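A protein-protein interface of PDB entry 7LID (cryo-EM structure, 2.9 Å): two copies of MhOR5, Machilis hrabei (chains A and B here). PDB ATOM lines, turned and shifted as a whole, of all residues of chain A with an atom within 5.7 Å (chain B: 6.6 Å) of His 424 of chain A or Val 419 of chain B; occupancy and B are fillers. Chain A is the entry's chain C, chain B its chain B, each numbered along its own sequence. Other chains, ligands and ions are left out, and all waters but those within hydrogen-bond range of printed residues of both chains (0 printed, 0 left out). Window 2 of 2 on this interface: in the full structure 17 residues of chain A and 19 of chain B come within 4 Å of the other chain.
The backbone carbonyl oxygen (O) of Val 419 of chain B lies within hydrogen-bond range of a ring nitrogen (NE2) of His 424 of chain A.
OG of Ser 416 of chain B is in hydrogen-bond range of O of Cys 326 of chain A (3.5 Å).
OG1 of Thr 428 of chain A lies within hydrogen-bond range of O of His 424 of chain A (2.5 Å).
SG of Cys 326 of chain A sits at hydrogen-bond distance from O of Ala 322 of chain A (3.2 Å).
Cys 326 of chain A touches Val 419 of chain B (SG to CG1, 3.8 Å).
Val 329 of chain A touches Tyr 414 of chain B (CG1 to CE1, 3.7 Å).
O of Ser 415 of chain B touches CG1 of Val 329 of chain A (3.3 Å).
CG2 of Val 329 of chain A touches CG2 of Val 419 of chain B (3.8 Å).
Thr 428 of chain A touches Val 419 of chain B.
His 424 of chain A touches just one residue of chain B: Val 419 (2.9 Å).
Of the printed residues of chain B, Cys 326 of chain A touches Ser 416 and Val 419.
Of the printed residues of chain A, Tyr 414 of chain B touches Val 329 (3.7 Å).
Leu 418 of chain B touches none of the printed residues of chain A.
The nearest residue of chain B that does not touch His 424 of chain A is Arg 426 of chain B (4.6 Å).
The nearest printed residue of chain A that does not touch Ser 416 of chain B is Val 329 of chain A (4.5 Å).
Of the 11 printed residues of chain B, 4 touch a printed residue of chain A.
Hydrophobic or aromatic side chains of chain B that line the printed part of chain A: Tyr 414 and Val 419.
Of the 12 printed residues of chain A, 4 touch a printed residue of chain B.
Printed residues of chain A that touch a printed residue of chain B: Cys 326, Val 329, His 424 and Thr 428.
Among the printed residues, 7 pairs touch across the chains.
3 positions are printed for both chains.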
ATOM      1  N   ALA A 322       2.300  -6.407   6.151  1.00  0.00           N
ATOM      2  CA  ALA A 322       3.407  -5.510   5.847  1.00  0.00           C
ATOM      3  C   ALA A 322       2.908  -4.108   5.533  1.00  0.00           C
ATOM      4  O   ALA A 322       3.378  -3.124   6.115  1.00  0.00           O
ATOM      5  CB  ALA A 322       4.220  -6.066   4.676  1.00  0.00           C
ATOM      6  N   LEU A 325       1.422  -1.841   8.322  1.00  0.00           N
ATOM      7  CA  LEU A 325       2.453  -1.371   9.238  1.00  0.00           C
ATOM      8  C   LEU A 325       3.331  -0.306   8.590  1.00  0.00           C
ATOM      9  O   LEU A 325       3.727   0.662   9.252  1.00  0.00           O
ATOM     10  CB  LEU A 325       3.294  -2.551   9.719  1.00  0.00           C
ATOM     11  CG  LEU A 325       2.591  -3.456  10.728  1.00  0.00           C
ATOM     12  CD1 LEU A 325       3.488  -4.606  11.118  1.00  0.00           C
ATOM     13  CD2 LEU A 325       2.180  -2.668  11.952  1.00  0.00           C
ATOM     14  N   CYS A 326       3.627  -0.453   7.295  1.00  0.00           N
ATOM     15  CA  CYS A 326       4.401   0.570   6.594  1.00  0.00           C
ATOM     16  C   CYS A 326       3.636   1.886   6.512  1.00  0.00           C
ATOM     17  O   CYS A 326       4.214   2.963   6.708  1.00  0.00           O
ATOM     18  CB  CYS A 326       4.791   0.082   5.199  1.00  0.00           C
ATOM     19  SG  CYS A 326       5.863  -1.367   5.178  1.00  0.00           S
ATOM     20  N   VAL A 329       3.702   3.492  10.059  1.00  0.00           N
ATOM     21  CA  VAL A 329       4.999   4.094  10.362  1.00  0.00           C
ATOM     22  C   VAL A 329       5.203   5.373   9.552  1.00  0.00           C
ATOM     23  O   VAL A 329       5.715   6.377  10.069  1.00  0.00           O
ATOM     24  CB  VAL A 329       6.122   3.064  10.128  1.00  0.00           C
ATOM     25  CG1 VAL A 329       7.487   3.709  10.173  1.00  0.00           C
ATOM     26  CG2 VAL A 329       6.052   1.977  11.173  1.00  0.00           C
ATOM     27  N   SER A 422       3.534 -12.735  15.016  1.00  0.00           N
ATOM     28  CA  SER A 422       4.837 -13.187  14.556  1.00  0.00           C
ATOM     29  C   SER A 422       5.944 -12.291  15.112  1.00  0.00           C
ATOM     30  O   SER A 422       5.702 -11.351  15.872  1.00  0.00           O
ATOM     31  CB  SER A 422       4.884 -13.209  13.030  1.00  0.00           C
ATOM     32  OG  SER A 422       4.304 -12.037  12.488  1.00  0.00           O
ATOM     33  N   ASP A 423       7.183 -12.593  14.721  1.00  0.00           N
ATOM     34  CA  ASP A 423       8.311 -11.788  15.184  1.00  0.00           C
ATOM     35  C   ASP A 423       8.386 -10.456  14.454  1.00  0.00           C
ATOM     36  O   ASP A 423       8.892  -9.473  15.011  1.00  0.00           O
ATOM     37  CB  ASP A 423       9.616 -12.562  15.015  1.00  0.00           C
ATOM     38  CG  ASP A 423       9.747 -13.699  16.004  1.00  0.00           C
ATOM     39  OD1 ASP A 423       9.194 -13.580  17.117  1.00  0.00           O
ATOM     40  OD2 ASP A 423      10.399 -14.711  15.672  1.00  0.00           O
ATOM     41  N   HIS A 424       7.887 -10.407  13.217  1.00  0.00           N
ATOM     42  CA  HIS A 424       7.855  -9.165  12.452  1.00  0.00           C
ATOM     43  C   HIS A 424       6.973  -8.125  13.132  1.00  0.00           C
ATOM     44  O   HIS A 424       7.386  -6.975  13.331  1.00  0.00           O
ATOM     45  CB  HIS A 424       7.350  -9.457  11.039  1.00  0.00           C
ATOM     46  CG  HIS A 424       7.701  -8.409  10.032  1.00  0.00           C
ATOM     47  ND1 HIS A 424       8.182  -8.719   8.780  1.00  0.00           N
ATOM     48  CD2 HIS A 424       7.624  -7.058  10.081  1.00  0.00           C
ATOM     49  CE1 HIS A 424       8.396  -7.606   8.104  1.00  0.00           C
ATOM     50  NE2 HIS A 424       8.066  -6.584   8.871  1.00  0.00           N
ATOM     51  N   VAL A 425       5.758  -8.522  13.509  1.00  0.00           N
ATOM     52  CA  VAL A 425       4.839  -7.605  14.175  1.00  0.00           C
ATOM     53  C   VAL A 425       5.345  -7.259  15.568  1.00  0.00           C
ATOM     54  O   VAL A 425       5.278  -6.102  15.999  1.00  0.00           O
ATOM     55  CB  VAL A 425       3.427  -8.214  14.215  1.00  0.00           C
ATOM     56  CG1 VAL A 425       2.451  -7.234  14.805  1.00  0.00           C
ATOM     57  CG2 VAL A 425       2.996  -8.618  12.821  1.00  0.00           C
ATOM     58  N   ARG A 426       5.885  -8.245  16.283  1.00  0.00           N
ATOM     59  CA  ARG A 426       6.388  -8.008  17.631  1.00  0.00           C
ATOM     60  C   ARG A 426       7.632  -7.133  17.655  1.00  0.00           C
ATOM     61  O   ARG A 426       7.922  -6.538  18.696  1.00  0.00           O
ATOM     62  CB  ARG A 426       6.683  -9.337  18.319  1.00  0.00           C
ATOM     63  CG  ARG A 426       6.163  -9.424  19.735  1.00  0.00           C
ATOM     64  CD  ARG A 426       6.378 -10.806  20.314  1.00  0.00           C
ATOM     65  NE  ARG A 426       5.821 -11.847  19.461  1.00  0.00           N
ATOM     66  CZ  ARG A 426       6.546 -12.779  18.855  1.00  0.00           C
ATOM     67  NH1 ARG A 426       5.960 -13.690  18.095  1.00  0.00           N
ATOM     68  NH2 ARG A 426       7.862 -12.796  19.008  1.00  0.00           N
ATOM     69  N   SER A 427       8.367  -7.038  16.550  1.00  0.00           N
ATOM     70  CA  SER A 427       9.469  -6.091  16.447  1.00  0.00           C
ATOM     71  C   SER A 427       9.023  -4.724  15.951  1.00  0.00           C
ATOM     72  O   SER A 427       9.540  -3.702  16.417  1.00  0.00           O
ATOM     73  CB  SER A 427      10.555  -6.640  15.521  1.00  0.00           C
ATOM     74  OG  SER A 427      11.392  -7.548  16.211  1.00  0.00           O
ATOM     75  N   THR A 428       8.049  -4.674  15.038  1.00  0.00           N
ATOM     76  CA  THR A 428       7.606  -3.388  14.510  1.00  0.00           C
ATOM     77  C   THR A 428       6.810  -2.603  15.547  1.00  0.00           C
ATOM     78  O   THR A 428       6.960  -1.379  15.654  1.00  0.00           O
ATOM     79  CB  THR A 428       6.781  -3.599  13.247  1.00  0.00           C
ATOM     80  OG1 THR A 428       7.379  -4.632  12.460  1.00  0.00           O
ATOM     81  CG2 THR A 428       6.746  -2.331  12.437  1.00  0.00           C
ATOM     82  N   ILE A 429       5.971  -3.288  16.333  1.00  0.00           N
ATOM     83  CA  ILE A 429       5.233  -2.615  17.401  1.00  0.00           C
ATOM     84  C   ILE A 429       6.193  -2.141  18.487  1.00  0.00           C
ATOM     85  O   ILE A 429       6.010  -1.066  19.076  1.00  0.00           O
ATOM     86  CB  ILE A 429       4.138  -3.548  17.955  1.00  0.00           C
ATOM     87  CG1 ILE A 429       3.119  -3.875  16.869  1.00  0.00           C
ATOM     88  CG2 ILE A 429       3.402  -2.914  19.109  1.00  0.00           C
ATOM     89  CD1 ILE A 429       2.453  -2.669  16.285  1.00  0.00           C
ATOM     90  N   TYR B 414      13.953   5.778  10.437  1.00  0.00           N
ATOM     91  CA  TYR B 414      12.640   5.304  10.862  1.00  0.00           C
ATOM     92  C   TYR B 414      11.680   5.616   9.721  1.00  0.00           C
ATOM     93  O   TYR B 414      11.222   6.751   9.587  1.00  0.00           O
ATOM     94  CB  TYR B 414      12.235   5.976  12.170  1.00  0.00           C
ATOM     95  CG  TYR B 414      10.894   5.583  12.736  1.00  0.00           C
ATOM     96  CD1 TYR B 414      10.516   4.255  12.830  1.00  0.00           C
ATOM     97  CD2 TYR B 414      10.025   6.547  13.224  1.00  0.00           C
ATOM     98  CE1 TYR B 414       9.296   3.904  13.367  1.00  0.00           C
ATOM     99  CE2 TYR B 414       8.808   6.204  13.760  1.00  0.00           C
ATOM    100  CZ  TYR B 414       8.450   4.883  13.829  1.00  0.00           C
ATOM    101  OH  TYR B 414       7.237   4.531  14.364  1.00  0.00           O
ATOM    102  N   SER B 415      11.440   4.637   8.858  1.00  0.00           N
ATOM    103  CA  SER B 415      10.577   4.810   7.694  1.00  0.00           C
ATOM    104  C   SER B 415       9.934   3.465   7.383  1.00  0.00           C
ATOM    105  O   SER B 415       9.900   2.566   8.228  1.00  0.00           O
ATOM    106  CB  SER B 415      11.363   5.346   6.486  1.00  0.00           C
ATOM    107  OG  SER B 415      12.346   6.286   6.857  1.00  0.00           O
ATOM    108  N   SER B 416       9.416   3.331   6.162  1.00  0.00           N
ATOM    109  CA  SER B 416       8.916   2.040   5.707  1.00  0.00           C
ATOM    110  C   SER B 416      10.051   1.085   5.379  1.00  0.00           C
ATOM    111  O   SER B 416       9.821  -0.119   5.229  1.00  0.00           O
ATOM    112  CB  SER B 416       8.026   2.227   4.486  1.00  0.00           C
ATOM    113  OG  SER B 416       7.075   3.241   4.719  1.00  0.00           O
ATOM    114  N   LYS B 417      11.273   1.601   5.245  1.00  0.00           N
ATOM    115  CA  LYS B 417      12.413   0.732   4.991  1.00  0.00           C
ATOM    116  C   LYS B 417      12.765  -0.090   6.223  1.00  0.00           C
ATOM    117  O   LYS B 417      13.122  -1.268   6.099  1.00  0.00           O
ATOM    118  CB  LYS B 417      13.602   1.570   4.532  1.00  0.00           C
ATOM    119  CG  LYS B 417      13.316   2.380   3.281  1.00  0.00           C
ATOM    120  CD  LYS B 417      13.276   1.499   2.048  1.00  0.00           C
ATOM    121  CE  LYS B 417      12.767   2.279   0.853  1.00  0.00           C
ATOM    122  NZ  LYS B 417      13.379   3.634   0.797  1.00  0.00           N
ATOM    123  N   LEU B 418      12.646   0.509   7.416  1.00  0.00           N
ATOM    124  CA  LEU B 418      12.895  -0.207   8.666  1.00  0.00           C
ATOM    125  C   LEU B 418      11.941  -1.377   8.848  1.00  0.00           C
ATOM    126  O   LEU B 418      12.342  -2.432   9.351  1.00  0.00           O
ATOM    127  CB  LEU B 418      12.770   0.749   9.850  1.00  0.00           C
ATOM    128  CG  LEU B 418      13.113   0.182  11.226  1.00  0.00           C
ATOM    129  CD1 LEU B 418      14.601   0.251  11.439  1.00  0.00           C
ATOM    130  CD2 LEU B 418      12.378   0.925  12.320  1.00  0.00           C
ATOM    131  N   VAL B 419      10.683  -1.215   8.434  1.00  0.00           N
ATOM    132  CA  VAL B 419       9.721  -2.307   8.477  1.00  0.00           C
ATOM    133  C   VAL B 419      10.037  -3.378   7.443  1.00  0.00           C
ATOM    134  O   VAL B 419       9.669  -4.543   7.631  1.00  0.00           O
ATOM    135  CB  VAL B 419       8.314  -1.695   8.299  1.00  0.00           C
ATOM    136  CG1 VAL B 419       7.209  -2.730   8.444  1.00  0.00           C
ATOM    137  CG2 VAL B 419       8.113  -0.567   9.287  1.00  0.00           C
ATOM    138  N   LEU B 420      10.779  -3.034   6.388  1.00  0.00           N
ATOM    139  CA  LEU B 420      11.092  -3.982   5.325  1.00  0.00           C
ATOM    140  C   LEU B 420      12.545  -4.442   5.363  1.00  0.00           C
ATOM    141  O   LEU B 420      13.014  -5.079   4.416  1.00  0.00           O
ATOM    142  CB  LEU B 420      10.767  -3.379   3.959  1.00  0.00           C
ATOM    143  CG  LEU B 420       9.291  -3.100   3.695  1.00  0.00           C
ATOM    144  CD1 LEU B 420       9.099  -2.561   2.293  1.00  0.00           C
ATOM    145  CD2 LEU B 420       8.479  -4.361   3.895  1.00  0.00           C
ATOM    146  N   ALA B 421      13.268  -4.136   6.432  1.00  0.00           N
ATOM    147  CA  ALA B 421      14.643  -4.584   6.565  1.00  0.00           C
ATOM    148  C   ALA B 421      14.698  -5.932   7.273  1.00  0.00           C
ATOM    149  O   ALA B 421      13.682  -6.469   7.718  1.00  0.00           O
ATOM    150  CB  ALA B 421      15.475  -3.554   7.324  1.00  0.00           C
ATOM    151  N   SER B 422      15.907  -6.477   7.374  1.00  0.00           N
ATOM    152  CA  SER B 422      16.097  -7.760   8.033  1.00  0.00           C
ATOM    153  C   SER B 422      16.042  -7.597   9.552  1.00  0.00           C
ATOM    154  O   SER B 422      15.825  -6.507  10.085  1.00  0.00           O
ATOM    155  CB  SER B 422      17.426  -8.382   7.610  1.00  0.00           C
ATOM    156  OG  SER B 422      18.462  -7.417   7.615  1.00  0.00           O
ATOM    157  N   ASP B 423      16.244  -8.712  10.259  1.00  0.00           N
ATOM    158  CA  ASP B 423      16.226  -8.662  11.719  1.00  0.00           C
ATOM    159  C   ASP B 423      17.505  -8.056  12.275  1.00  0.00           C
ATOM    160  O   ASP B 423      17.489  -7.467  13.363  1.00  0.00           O
ATOM    161  CB  ASP B 423      16.007 -10.059  12.291  1.00  0.00           C
ATOM    162  CG  ASP B 423      14.593 -10.556  12.079  1.00  0.00           C
ATOM    163  OD1 ASP B 423      13.672  -9.716  12.032  1.00  0.00           O
ATOM    164  OD2 ASP B 423      14.401 -11.785  11.960  1.00  0.00           O
ATOM    165  N   ARG B 426      16.954  -4.299  12.006  1.00  0.00           N
ATOM    166  CA  ARG B 426      15.887  -3.929  12.927  1.00  0.00           C
ATOM    167  C   ARG B 426      16.289  -4.067  14.387  1.00  0.00           C
ATOM    168  O   ARG B 426      15.661  -3.435  15.242  1.00  0.00           O
ATOM    169  CB  ARG B 426      14.646  -4.774  12.655  1.00  0.00           C
ATOM    170  CG  ARG B 426      13.361  -3.981  12.612  1.00  0.00           C
ATOM    171  CD  ARG B 426      12.190  -4.855  12.216  1.00  0.00           C
ATOM    172  NE  ARG B 426      12.438  -5.566  10.968  1.00  0.00           N
ATOM    173  CZ  ARG B 426      12.524  -6.887  10.869  1.00  0.00           C
ATOM    174  NH1 ARG B 426      12.754  -7.453   9.695  1.00  0.00           N
ATOM    175  NH2 ARG B 426      12.386  -7.641  11.948  1.00  0.00           N
